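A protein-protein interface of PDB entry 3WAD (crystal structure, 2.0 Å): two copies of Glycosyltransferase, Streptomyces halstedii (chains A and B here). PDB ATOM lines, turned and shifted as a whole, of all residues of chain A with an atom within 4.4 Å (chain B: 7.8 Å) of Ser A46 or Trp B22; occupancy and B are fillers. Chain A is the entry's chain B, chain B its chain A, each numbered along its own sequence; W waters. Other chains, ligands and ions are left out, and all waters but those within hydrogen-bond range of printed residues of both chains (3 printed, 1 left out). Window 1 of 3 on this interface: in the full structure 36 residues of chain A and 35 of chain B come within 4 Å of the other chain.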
ATOM      1  N   LEU A  14     -10.263  21.026  16.986  1.00  0.00           N
ATOM      2  CA  LEU A  14     -10.636  19.877  16.118  1.00  0.00           C
ATOM      3  C   LEU A  14     -10.270  18.542  16.694  1.00  0.00           C
ATOM      4  O   LEU A  14     -11.173  17.707  16.839  1.00  0.00           O
ATOM      5  CB  LEU A  14     -10.138  20.012  14.686  1.00  0.00           C
ATOM      6  CG  LEU A  14     -10.312  18.720  13.867  1.00  0.00           C
ATOM      7  CD1 LEU A  14     -11.786  18.232  13.743  1.00  0.00           C
ATOM      8  CD2 LEU A  14      -9.590  18.790  12.501  1.00  0.00           C
ATOM      9  N   TYR A  15      -8.974  18.297  17.003  1.00  0.00           N
ATOM     10  CA  TYR A  15      -8.522  17.010  17.552  1.00  0.00           C
ATOM     11  C   TYR A  15      -9.235  16.584  18.832  1.00  0.00           C
ATOM     12  O   TYR A  15      -9.340  15.368  19.140  1.00  0.00           O
ATOM     13  CB  TYR A  15      -7.030  17.095  17.915  1.00  0.00           C
ATOM     14  CG  TYR A  15      -6.134  17.147  16.718  1.00  0.00           C
ATOM     15  CD1 TYR A  15      -6.661  17.219  15.405  1.00  0.00           C
ATOM     16  CD2 TYR A  15      -4.749  17.086  16.905  1.00  0.00           C
ATOM     17  CE1 TYR A  15      -5.817  17.239  14.306  1.00  0.00           C
ATOM     18  CE2 TYR A  15      -3.906  17.136  15.843  1.00  0.00           C
ATOM     19  CZ  TYR A  15      -4.431  17.198  14.553  1.00  0.00           C
ATOM     20  OH  TYR A  15      -3.516  17.233  13.531  1.00  0.00           O
ATOM     21  N   VAL A  18     -12.171  14.525  17.554  1.00  0.00           N
ATOM     22  CA  VAL A  18     -11.958  13.555  16.507  1.00  0.00           C
ATOM     23  C   VAL A  18     -12.321  12.107  16.894  1.00  0.00           C
ATOM     24  O   VAL A  18     -12.974  11.452  16.132  1.00  0.00           O
ATOM     25  CB  VAL A  18     -10.520  13.655  15.890  1.00  0.00           C
ATOM     26  CG1 VAL A  18     -10.022  12.314  15.240  1.00  0.00           C
ATOM     27  CG2 VAL A  18     -10.473  14.813  14.870  1.00  0.00           C
ATOM     28  N   TRP A  22     -15.194   9.780  15.188  1.00  0.00           N
ATOM     29  CA  TRP A  22     -14.992   8.436  14.708  1.00  0.00           C
ATOM     30  C   TRP A  22     -15.780   7.314  15.441  1.00  0.00           C
ATOM     31  O   TRP A  22     -16.193   6.351  14.771  1.00  0.00           O
ATOM     32  CB  TRP A  22     -13.517   8.071  14.711  1.00  0.00           C
ATOM     33  CG  TRP A  22     -12.880   8.336  13.343  1.00  0.00           C
ATOM     34  CD1 TRP A  22     -12.003   9.362  13.010  1.00  0.00           C
ATOM     35  CD2 TRP A  22     -13.093   7.589  12.129  1.00  0.00           C
ATOM     36  NE1 TRP A  22     -11.649   9.267  11.674  1.00  0.00           N
ATOM     37  CE2 TRP A  22     -12.327   8.228  11.098  1.00  0.00           C
ATOM     38  CE3 TRP A  22     -13.857   6.446  11.804  1.00  0.00           C
ATOM     39  CZ2 TRP A  22     -12.251   7.727   9.782  1.00  0.00           C
ATOM     40  CZ3 TRP A  22     -13.796   5.948  10.475  1.00  0.00           C
ATOM     41  CH2 TRP A  22     -12.977   6.591   9.483  1.00  0.00           C
ATOM     42  N   THR A  26     -18.228   4.746  13.481  1.00  0.00           N
ATOM     43  CA  THR A  26     -18.088   3.303  13.382  1.00  0.00           C
ATOM     44  C   THR A  26     -19.278   2.559  14.028  1.00  0.00           C
ATOM     45  O   THR A  26     -19.432   1.345  13.845  1.00  0.00           O
ATOM     46  CB  THR A  26     -16.750   2.812  13.931  1.00  0.00           C
ATOM     47  OG1 THR A  26     -16.585   3.247  15.303  1.00  0.00           O
ATOM     48  CG2 THR A  26     -15.551   3.373  12.963  1.00  0.00           C
ATOM     49  N   ALA A  42      -7.067  19.804   7.870  1.00  0.00           N
ATOM     50  CA  ALA A  42      -6.951  19.131   9.159  1.00  0.00           C
ATOM     51  C   ALA A  42      -8.104  18.088   9.315  1.00  0.00           C
ATOM     52  O   ALA A  42      -7.886  17.020   9.882  1.00  0.00           O
ATOM     53  CB  ALA A  42      -6.999  20.125  10.334  1.00  0.00           C
ATOM     54  N   ILE A  43      -9.317  18.424   8.857  1.00  0.00           N
ATOM     55  CA  ILE A  43     -10.412  17.471   9.029  1.00  0.00           C
ATOM     56  C   ILE A  43     -10.114  16.265   8.152  1.00  0.00           C
ATOM     57  O   ILE A  43     -10.284  15.118   8.568  1.00  0.00           O
ATOM     58  CB  ILE A  43     -11.782  18.079   8.645  1.00  0.00           C
ATOM     59  CG1 ILE A  43     -12.195  19.193   9.636  1.00  0.00           C
ATOM     60  CG2 ILE A  43     -12.829  16.950   8.648  1.00  0.00           C
ATOM     61  CD1 ILE A  43     -13.162  20.228   9.134  1.00  0.00           C
ATOM     62  N   SER A  44      -9.658  16.525   6.924  1.00  0.00           N
ATOM     63  CA  SER A  44      -9.166  15.420   6.079  1.00  0.00           C
ATOM     64  C   SER A  44      -8.086  14.562   6.626  1.00  0.00           C
ATOM     65  O   SER A  44      -8.146  13.320   6.475  1.00  0.00           O
ATOM     66  CB  SER A  44      -8.744  15.933   4.695  1.00  0.00           C
ATOM     67  OG  SER A  44      -9.924  16.234   4.029  1.00  0.00           O
ATOM     68  N   ASP A  45      -7.095  15.175   7.249  1.00  0.00           N
ATOM     69  CA  ASP A  45      -5.967  14.448   7.792  1.00  0.00           C
ATOM     70  C   ASP A  45      -6.404  13.616   8.991  1.00  0.00           C
ATOM     71  O   ASP A  45      -5.597  12.856   9.514  1.00  0.00           O
ATOM     72  CB  ASP A  45      -4.878  15.374   8.302  1.00  0.00           C
ATOM     73  CG  ASP A  45      -4.146  16.153   7.173  1.00  0.00           C
ATOM     74  OD1 ASP A  45      -4.210  15.726   6.002  1.00  0.00           O
ATOM     75  OD2 ASP A  45      -3.493  17.176   7.533  1.00  0.00           O
ATOM     76  N   SER A  46      -7.615  13.874   9.500  1.00  0.00           N
ATOM     77  CA  SER A  46      -8.134  13.129  10.641  1.00  0.00           C
ATOM     78  C   SER A  46      -9.028  11.938  10.187  1.00  0.00           C
ATOM     79  O   SER A  46      -9.537  11.213  11.009  1.00  0.00           O
ATOM     80  CB  SER A  46      -8.940  14.004  11.570  1.00  0.00           C
ATOM     81  OG  SER A  46      -8.199  15.092  11.992  1.00  0.00           O
ATOM     82  N   GLY A  47      -9.224  11.816   8.880  1.00  0.00           N
ATOM     83  CA  GLY A  47     -10.074  10.811   8.266  1.00  0.00           C
ATOM     84  C   GLY A  47     -11.556  11.113   8.243  1.00  0.00           C
ATOM     85  O   GLY A  47     -12.337  10.174   8.042  1.00  0.00           O
ATOM     86  N   LEU A  48     -11.969  12.382   8.371  1.00  0.00           N
ATOM     87  CA  LEU A  48     -13.386  12.687   8.560  1.00  0.00           C
ATOM     88  C   LEU A  48     -13.922  13.536   7.400  1.00  0.00           C
ATOM     89  O   LEU A  48     -13.138  13.956   6.540  1.00  0.00           O
ATOM     90  CB  LEU A  48     -13.605  13.405   9.931  1.00  0.00           C
ATOM     91  CG  LEU A  48     -13.209  12.625  11.150  1.00  0.00           C
ATOM     92  CD1 LEU A  48     -13.086  13.414  12.501  1.00  0.00           C
ATOM     93  CD2 LEU A  48     -14.205  11.379  11.286  1.00  0.00           C
ATOM     94  N   PHE A 229      -6.482  12.673  20.867  1.00  0.00           N
ATOM     95  CA  PHE A 229      -6.056  12.424  19.482  1.00  0.00           C
ATOM     96  C   PHE A 229      -4.814  13.291  19.267  1.00  0.00           C
ATOM     97  O   PHE A 229      -4.903  14.547  19.349  1.00  0.00           O
ATOM     98  CB  PHE A 229      -7.147  12.819  18.459  1.00  0.00           C
ATOM     99  CG  PHE A 229      -6.711  12.657  16.998  1.00  0.00           C
ATOM    100  CD1 PHE A 229      -6.269  11.439  16.544  1.00  0.00           C
ATOM    101  CD2 PHE A 229      -6.790  13.726  16.104  1.00  0.00           C
ATOM    102  CE1 PHE A 229      -5.875  11.257  15.220  1.00  0.00           C
ATOM    103  CE2 PHE A 229      -6.391  13.575  14.774  1.00  0.00           C
ATOM    104  CZ  PHE A 229      -5.917  12.309  14.325  1.00  0.00           C
ATOM    105  N   MET B   5      -1.994  -4.028  12.488  1.00  0.00           N
ATOM    106  CA  MET B   5      -2.611  -4.215  11.207  1.00  0.00           C
ATOM    107  C   MET B   5      -1.580  -4.106  10.097  1.00  0.00           C
ATOM    108  O   MET B   5      -0.596  -3.382  10.205  1.00  0.00           O
ATOM    109  CB  MET B   5      -3.754  -3.218  11.034  1.00  0.00           C
ATOM    110  CG  MET B   5      -4.682  -3.254  12.263  1.00  0.00           C
ATOM    111  SD  MET B   5      -6.122  -2.235  12.122  1.00  0.00           S
ATOM    112  CE  MET B   5      -7.085  -2.755  10.689  1.00  0.00           C
ATOM    113  N   MET B  17      -9.616  -1.125   5.269  1.00  0.00           N
ATOM    114  CA  MET B  17      -9.425  -1.421   6.664  1.00  0.00           C
ATOM    115  C   MET B  17      -9.366  -0.257   7.621  1.00  0.00           C
ATOM    116  O   MET B  17      -9.229  -0.502   8.838  1.00  0.00           O
ATOM    117  CB  MET B  17      -8.254  -2.361   6.847  1.00  0.00           C
ATOM    118  CG  MET B  17      -6.934  -1.653   6.685  1.00  0.00           C
ATOM    119  SD  MET B  17      -5.534  -2.638   7.313  1.00  0.00           S
ATOM    120  CE  MET B  17      -5.802  -4.221   6.518  1.00  0.00           C
ATOM    121  N   VAL B  18      -9.448   0.986   7.095  1.00  0.00           N
ATOM    122  CA  VAL B  18      -9.438   2.215   7.938  1.00  0.00           C
ATOM    123  C   VAL B  18     -10.583   2.324   8.987  1.00  0.00           C
ATOM    124  O   VAL B  18     -10.329   2.597  10.152  1.00  0.00           O
ATOM    125  CB  VAL B  18      -9.440   3.503   7.064  1.00  0.00           C
ATOM    126  CG1 VAL B  18      -9.783   4.784   7.850  1.00  0.00           C
ATOM    127  CG2 VAL B  18      -8.021   3.695   6.355  1.00  0.00           C
ATOM    128  N   PRO B  19     -11.856   2.141   8.567  1.00  0.00           N
ATOM    129  CA  PRO B  19     -12.875   2.286   9.651  1.00  0.00           C
ATOM    130  C   PRO B  19     -12.721   1.246  10.784  1.00  0.00           C
ATOM    131  O   PRO B  19     -12.851   1.630  11.964  1.00  0.00           O
ATOM    132  CB  PRO B  19     -14.221   2.169   8.899  1.00  0.00           C
ATOM    133  CG  PRO B  19     -13.810   2.572   7.420  1.00  0.00           C
ATOM    134  CD  PRO B  19     -12.465   1.983   7.227  1.00  0.00           C
ATOM    135  N   LEU B  20     -12.370   0.005  10.440  1.00  0.00           N
ATOM    136  CA  LEU B  20     -12.043  -1.020  11.466  1.00  0.00           C
ATOM    137  C   LEU B  20     -10.917  -0.538  12.381  1.00  0.00           C
ATOM    138  O   LEU B  20     -11.013  -0.615  13.632  1.00  0.00           O
ATOM    139  CB  LEU B  20     -11.671  -2.332  10.835  1.00  0.00           C
ATOM    140  CG  LEU B  20     -11.444  -3.542  11.799  1.00  0.00           C
ATOM    141  CD1 LEU B  20     -12.757  -3.874  12.635  1.00  0.00           C
ATOM    142  CD2 LEU B  20     -10.923  -4.758  11.072  1.00  0.00           C
ATOM    143  N   ALA B  21      -9.837   0.008  11.767  1.00  0.00           N
ATOM    144  CA  ALA B  21      -8.730   0.546  12.552  1.00  0.00           C
ATOM    145  C   ALA B  21      -9.248   1.617  13.515  1.00  0.00           C
ATOM    146  O   ALA B  21      -8.853   1.715  14.657  1.00  0.00           O
ATOM    147  CB  ALA B  21      -7.716   1.185  11.574  1.00  0.00           C
ATOM    148  N   TRP B  22     -10.108   2.468  13.025  1.00  0.00           N
ATOM    149  CA  TRP B  22     -10.683   3.435  13.900  1.00  0.00           C
ATOM    150  C   TRP B  22     -11.725   2.925  14.985  1.00  0.00           C
ATOM    151  O   TRP B  22     -11.881   3.553  16.035  1.00  0.00           O
ATOM    152  CB  TRP B  22     -11.310   4.486  13.087  1.00  0.00           C
ATOM    153  CG  TRP B  22     -10.356   5.674  12.821  1.00  0.00           C
ATOM    154  CD1 TRP B  22      -9.732   6.011  11.618  1.00  0.00           C
ATOM    155  CD2 TRP B  22      -9.902   6.610  13.798  1.00  0.00           C
ATOM    156  NE1 TRP B  22      -8.955   7.154  11.805  1.00  0.00           N
ATOM    157  CE2 TRP B  22      -9.020   7.520  13.133  1.00  0.00           C
ATOM    158  CE3 TRP B  22     -10.190   6.796  15.185  1.00  0.00           C
ATOM    159  CZ2 TRP B  22      -8.446   8.588  13.790  1.00  0.00           C
ATOM    160  CZ3 TRP B  22      -9.611   7.833  15.839  1.00  0.00           C
ATOM    161  CH2 TRP B  22      -8.737   8.747  15.144  1.00  0.00           C
ATOM    162  N   ALA B  23     -12.519   1.911  14.645  1.00  0.00           N
ATOM    163  CA  ALA B  23     -13.346   1.158  15.645  1.00  0.00           C
ATOM    164  C   ALA B  23     -12.470   0.622  16.760  1.00  0.00           C
ATOM    165  O   ALA B  23     -12.763   0.803  17.985  1.00  0.00           O
ATOM    166  CB  ALA B  23     -14.083  -0.008  14.943  1.00  0.00           C
ATOM    167  N   LEU B  24     -11.371  -0.004  16.371  1.00  0.00           N
ATOM    168  CA  LEU B  24     -10.455  -0.470  17.350  1.00  0.00           C
ATOM    169  C   LEU B  24      -9.871   0.647  18.194  1.00  0.00           C
ATOM    170  O   LEU B  24      -9.713   0.490  19.421  1.00  0.00           O
ATOM    171  CB  LEU B  24      -9.349  -1.327  16.722  1.00  0.00           C
ATOM    172  CG  LEU B  24      -9.830  -2.669  16.150  1.00  0.00           C
ATOM    173  CD1 LEU B  24      -8.797  -3.184  15.233  1.00  0.00           C
ATOM    174  CD2 LEU B  24     -10.032  -3.705  17.287  1.00  0.00           C
ATOM    175  N   THR B  25      -9.588   1.794  17.558  1.00  0.00           N
ATOM    176  CA  THR B  25      -8.969   2.917  18.225  1.00  0.00           C
ATOM    177  C   THR B  25      -9.847   3.511  19.292  1.00  0.00           C
ATOM    178  O   THR B  25      -9.392   3.644  20.442  1.00  0.00           O
ATOM    179  CB  THR B  25      -8.544   3.989  17.205  1.00  0.00           C
ATOM    180  OG1 THR B  25      -7.646   3.317  16.337  1.00  0.00           O
ATOM    181  CG2 THR B  25      -7.753   5.020  17.907  1.00  0.00           C
ATOM    182  N   THR B  26     -11.095   3.798  18.937  1.00  0.00           N
ATOM    183  CA  THR B  26     -11.993   4.476  19.876  1.00  0.00           C
ATOM    184  C   THR B  26     -12.496   3.559  21.015  1.00  0.00           C
ATOM    185  O   THR B  26     -13.039   4.057  22.037  1.00  0.00           O
ATOM    186  CB  THR B  26     -13.159   5.121  19.227  1.00  0.00           C
ATOM    187  OG1 THR B  26     -13.897   4.161  18.481  1.00  0.00           O
ATOM    188  CG2 THR B  26     -12.689   6.288  18.327  1.00  0.00           C
ATOM    189  N   ALA B  27     -12.315   2.258  20.840  1.00  0.00           N
ATOM    190  CA  ALA B  27     -12.488   1.269  21.903  1.00  0.00           C
ATOM    191  C   ALA B  27     -11.284   1.210  22.830  1.00  0.00           C
ATOM    192  O   ALA B  27     -11.281   0.472  23.787  1.00  0.00           O
ATOM    193  CB  ALA B  27     -12.754  -0.170  21.268  1.00  0.00           C
ATOM    194  N   GLY B  28     -10.267   2.023  22.574  1.00  0.00           N
ATOM    195  CA  GLY B  28      -9.153   2.184  23.509  1.00  0.00           C
ATOM    196  C   GLY B  28      -7.962   1.324  23.189  1.00  0.00           C
ATOM    197  O   GLY B  28      -6.993   1.394  23.892  1.00  0.00           O
ATOM    198  N   HIS B  29      -8.004   0.509  22.144  1.00  0.00           N
ATOM    199  CA  HIS B  29      -6.852  -0.319  21.828  1.00  0.00           C
ATOM    200  C   HIS B  29      -5.754   0.475  21.105  1.00  0.00           C
ATOM    201  O   HIS B  29      -6.034   1.456  20.377  1.00  0.00           O
ATOM    202  CB  HIS B  29      -7.238  -1.569  21.011  1.00  0.00           C
ATOM    203  CG  HIS B  29      -8.380  -2.334  21.616  1.00  0.00           C
ATOM    204  ND1 HIS B  29      -8.222  -3.107  22.751  1.00  0.00           N
ATOM    205  CD2 HIS B  29      -9.700  -2.363  21.313  1.00  0.00           C
ATOM    206  CE1 HIS B  29      -9.396  -3.625  23.097  1.00  0.00           C
ATOM    207  NE2 HIS B  29     -10.308  -3.205  22.234  1.00  0.00           N
ATOM    208  N   VAL B  31      -3.387   0.761  18.145  1.00  0.00           N
ATOM    209  CA  VAL B  31      -3.419   0.264  16.782  1.00  0.00           C
ATOM    210  C   VAL B  31      -2.206   0.783  15.988  1.00  0.00           C
ATOM    211  O   VAL B  31      -1.979   1.995  15.965  1.00  0.00           O
ATOM    212  CB  VAL B  31      -4.657   0.728  16.072  1.00  0.00           C
ATOM    213  CG1 VAL B  31      -4.652   0.224  14.657  1.00  0.00           C
ATOM    214  CG2 VAL B  31      -5.947   0.272  16.828  1.00  0.00           C
ATOM    215  N   ILE B  33      -0.557   0.580  11.967  1.00  0.00           N
ATOM    216  CA  ILE B  33      -0.710   0.051  10.567  1.00  0.00           C
ATOM    217  C   ILE B  33       0.646  -0.010   9.947  1.00  0.00           C
ATOM    218  O   ILE B  33       1.284   1.028   9.689  1.00  0.00           O
ATOM    219  CB  ILE B  33      -1.608   0.934   9.666  1.00  0.00           C
ATOM    220  CG1 ILE B  33      -2.741   1.502  10.464  1.00  0.00           C
ATOM    221  CG2 ILE B  33      -2.041   0.188   8.348  1.00  0.00           C
ATOM    222  CD1 ILE B  33      -3.783   0.491  10.857  1.00  0.00           C
ATOM    223  N   ILE B  43      -1.706   6.529   5.246  1.00  0.00           N
ATOM    224  CA  ILE B  43      -2.083   6.007   6.556  1.00  0.00           C
ATOM    225  C   ILE B  43      -2.205   7.112   7.537  1.00  0.00           C
ATOM    226  O   ILE B  43      -3.213   7.207   8.274  1.00  0.00           O
ATOM    227  CB  ILE B  43      -1.069   4.992   7.132  1.00  0.00           C
ATOM    228  CG1 ILE B  43      -1.090   3.691   6.350  1.00  0.00           C
ATOM    229  CG2 ILE B  43      -1.387   4.761   8.645  1.00  0.00           C
ATOM    230  CD1 ILE B  43       0.192   2.812   6.622  1.00  0.00           C
ATOM    231  N   SER B  44      -1.177   7.963   7.561  1.00  0.00           N
ATOM    232  CA  SER B  44      -1.209   9.121   8.430  1.00  0.00           C
ATOM    233  C   SER B  44      -2.280  10.187   8.044  1.00  0.00           C
ATOM    234  O   SER B  44      -2.895  10.784   8.930  1.00  0.00           O
ATOM    235  CB  SER B  44       0.225   9.718   8.531  1.00  0.00           C
ATOM    236  OG  SER B  44       0.209  10.879   7.784  1.00  0.00           O
ATOM    237  N   ASP B  45      -2.529  10.369   6.744  1.00  0.00           N
ATOM    238  CA  ASP B  45      -3.638  11.151   6.223  1.00  0.00           C
ATOM    239  C   ASP B  45      -5.057  10.597   6.430  1.00  0.00           C
ATOM    240  O   ASP B  45      -6.000  11.244   6.067  1.00  0.00           O
ATOM    241  CB  ASP B  45      -3.486  11.215   4.715  1.00  0.00           C
ATOM    242  CG  ASP B  45      -2.421  12.275   4.234  1.00  0.00           C
ATOM    243  OD1 ASP B  45      -1.674  12.852   5.076  1.00  0.00           O
ATOM    244  OD2 ASP B  45      -2.352  12.445   2.988  1.00  0.00           O
ATOM    245  N   SER B  46      -5.187   9.345   6.897  1.00  0.00           N
ATOM    246  CA  SER B  46      -6.487   8.796   7.381  1.00  0.00           C
ATOM    247  C   SER B  46      -6.554   8.913   8.929  1.00  0.00           C
ATOM    248  O   SER B  46      -7.434   8.323   9.547  1.00  0.00           O
ATOM    249  CB  SER B  46      -6.578   7.324   7.009  1.00  0.00           C
ATOM    250  OG  SER B  46      -6.373   7.150   5.620  1.00  0.00           O
ATOM    251  N   GLY B  47      -5.616   9.658   9.533  1.00  0.00           N
ATOM    252  CA  GLY B  47      -5.595   9.855  10.985  1.00  0.00           C
ATOM    253  C   GLY B  47      -4.975   8.770  11.829  1.00  0.00           C
ATOM    254  O   GLY B  47      -5.152   8.739  13.062  1.00  0.00           O
ATOM    255  N   LEU B  48      -4.263   7.841  11.234  1.00  0.00           N
ATOM    256  CA  LEU B  48      -3.799   6.682  12.032  1.00  0.00           C
ATOM    257  C   LEU B  48      -2.291   6.697  12.099  1.00  0.00           C
ATOM    258  O   LEU B  48      -1.675   7.541  11.456  1.00  0.00           O
ATOM    259  CB  LEU B  48      -4.266   5.396  11.328  1.00  0.00           C
ATOM    260  CG  LEU B  48      -5.783   5.181  11.183  1.00  0.00           C
ATOM    261  CD1 LEU B  48      -6.145   4.168  10.020  1.00  0.00           C
ATOM    262  CD2 LEU B  48      -6.433   4.844  12.489  1.00  0.00           C
ATOM    263  N   THR B  49      -1.725   5.766  12.841  1.00  0.00           N
ATOM    264  CA  THR B  49      -0.296   5.669  13.149  1.00  0.00           C
ATOM    265  C   THR B  49       0.341   4.627  12.282  1.00  0.00           C
ATOM    266  O   THR B  49       0.032   3.403  12.412  1.00  0.00           O
ATOM    267  CB  THR B  49      -0.063   5.290  14.656  1.00  0.00           C
ATOM    268  OG1 THR B  49      -0.667   6.287  15.458  1.00  0.00           O
ATOM    269  CG2 THR B  49       1.441   5.234  15.024  1.00  0.00           C
ATOM    270  N   PHE B 229     -14.580   3.545   3.062  1.00  0.00           N
ATOM    271  CA  PHE B 229     -13.909   4.831   3.304  1.00  0.00           C
ATOM    272  C   PHE B 229     -13.180   5.098   2.012  1.00  0.00           C
ATOM    273  O   PHE B 229     -12.712   4.167   1.417  1.00  0.00           O
ATOM    274  CB  PHE B 229     -12.905   4.638   4.435  1.00  0.00           C
ATOM    275  CG  PHE B 229     -12.083   5.862   4.743  1.00  0.00           C
ATOM    276  CD1 PHE B 229     -12.592   6.866   5.558  1.00  0.00           C
ATOM    277  CD2 PHE B 229     -10.759   5.969   4.268  1.00  0.00           C
ATOM    278  CE1 PHE B 229     -11.781   8.005   5.843  1.00  0.00           C
ATOM    279  CE2 PHE B 229      -9.958   7.074   4.570  1.00  0.00           C
ATOM    280  CZ  PHE B 229     -10.464   8.078   5.342  1.00  0.00           C
ATOM    281  N   LEU B 402     -19.737  -2.183  13.485  1.00  0.00           N
ATOM    282  CA  LEU B 402     -18.289  -2.318  13.798  1.00  0.00           C
ATOM    283  C   LEU B 402     -17.996  -2.551  15.269  1.00  0.00           C
ATOM    284  O   LEU B 402     -16.998  -3.184  15.631  1.00  0.00           O
ATOM    285  CB  LEU B 402     -17.422  -1.170  13.216  1.00  0.00           C
ATOM    286  CG  LEU B 402     -17.012  -1.496  11.782  1.00  0.00           C
ATOM    287  CD1 LEU B 402     -18.171  -1.535  10.745  1.00  0.00           C
ATOM    288  CD2 LEU B 402     -15.933  -0.417  11.257  1.00  0.00           C
ATOM    289  N   VAL B 406     -15.509  -5.412  16.777  1.00  0.00           N
ATOM    290  CA  VAL B 406     -14.413  -5.202  17.764  1.00  0.00           C
ATOM    291  C   VAL B 406     -14.481  -6.219  18.951  1.00  0.00           C
ATOM    292  O   VAL B 406     -13.490  -6.872  19.320  1.00  0.00           O
ATOM    293  CB  VAL B 406     -14.397  -3.658  18.207  1.00  0.00           C
ATOM    294  CG1 VAL B 406     -13.531  -3.399  19.431  1.00  0.00           C
ATOM    295  CG2 VAL B 406     -13.940  -2.825  17.011  1.00  0.00           C
HETATM  296  O   HOH W   1      -9.037  11.332   4.827  1.00  0.00           O
HETATM  297  O   HOH W   2     -14.354   4.337  15.942  1.00  0.00           O
HETATM  298  O   HOH W   3     -21.261  -0.207  12.645  1.00  0.00           O
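N of Gly B47 sits at hydrogen-bond distance from O of Asp A45 (3.2 Å). NE1 of Trp B22 lies close to NE1 of Trp A22 (3.4 Å). The backbone carbonyl oxygen of Ser A44 sits close to the backbone carbonyl oxygen of Asp B45, 3.0 Å away. The backbone carbonyl oxygen of Ser B44 lies close to the backbone carbonyl oxygen of Asp A45, at 3.5 Å.
The side-chain hydroxyl (OG1) of Thr B26 sits at hydrogen-bond distance from the backbone carbonyl oxygen (O) of Trp B22, 3.2 Å away. The indole nitrogen (NE1) of Trp B22 is in hydrogen-bond range of the backbone carbonyl oxygen (O) of Ser B46 (3.0 Å). The backbone carbonyl oxygen of Trp A22 is in hydrogen-bond range of the side-chain hydroxyl of Thr A26, 3.2 Å away. NE1 of Trp A22 lies within hydrogen-bond range of O of Ser A46, at 2.9 Å. The side-chain hydroxyl of Ser A46 sits at hydrogen-bond distance from the backbone carbonyl oxygen of Ala A42 (2.9 Å).
Trp B22 touches Val A18 (CH2 to CG1, 3.8 Å). Pro B19 touches Trp A22 (CA to CZ3, 3.9 Å). O of Pro B19 touches CG2 of Thr A26 (3.4 Å). CG2 of Thr A26 touches N of Ala B23, 3.8 Å away. Thr A26 touches Leu B402. CA of Asp A45 touches O of Asp B45, 3.6 Å away. Trp B22 touches Ser A46 (CZ2 to O, 3.98 Å). O of Ser B46 touches O of Ser A46, 3.9 Å away. CH2 of Trp B22 touches CE1 of Phe A229, 3.8 Å away. CE1 of Phe A229 touches O of Gly B47 (3.4 Å).
Of chain B, only Trp B22 (3.98 Å) and Ser B46 (3.9 Å) come within 4 Å of Ser A46. Of the printed residues of chain A, Pro B19 touches Trp A22 and Thr A26. Of chain A, only Val A18 (3.8 Å), Trp A22 (3.4 Å), Ser A46 (3.98 Å) and Phe A229 (3.8 Å) come within 4 Å of Trp B22. Of the printed residues of chain A, Ser B44 touches Asp A45 (3.5 Å). Of the printed residues of chain A, Gly B47 touches Asp A45 and Phe A229. Printed residues of chain A within 4 Å of Leu B402: Thr A26 (3.3 Å). The nearest residue of chain B that does not touch Ser A46 is Gly B47 (4.1 Å). The nearest printed residue of chain A that does not touch Trp B22 is Thr A26 (4.4 Å).
Hydrophobic or aromatic side chains of chain A that line the printed part of chain B: Val A18, Trp A22 and Phe A229. Of the 26 printed residues of chain B, 9 touch a printed residue of chain A. Printed residues of chain B that touch a printed residue of chain A: Pro B19, Trp B22, Ala B23, Ser B44, Asp B45, Ser B46, Gly B47, Phe B229 and Leu B402. Hydrophobic or aromatic side chains of chain B that line the printed part of chain A: Trp B22, Phe B229 and Leu B402. Among the printed residues, no Asp or Glu carboxylate lies within 4 Å of a Lys or Arg side-chain nitrogen of the other chain.
Ser A44 touches Asp B45, and with the chains exchanged Asp A45 touches Ser B44. Asp B45 touches its own counterpart, Asp A45. Asp A45 touches Gly B47, but with the chains exchanged Gly A47 does not touch Asp B45 (4.3 Å). Ser B46 touches its own counterpart, Ser A46. 10 positions are printed for both chains.
Water W2 lies within hydrogen-bond range of OG1 of Thr A26 (2.6 Å), OG1 of Thr B26 (2.6 Å), O of Trp B22 (2.6 Å), O of Trp A22 (3.0 Å) and N of Ala B23 (3.3 Å). Water W3 lies within hydrogen-bond range of N of Leu B402 and O of Thr A26. Water W1 lies within hydrogen-bond range of the backbone carbonyl oxygen of Ser A44 (2.7 Å) and the backbone carbonyl oxygen of Asp B45 (3.3 Å).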
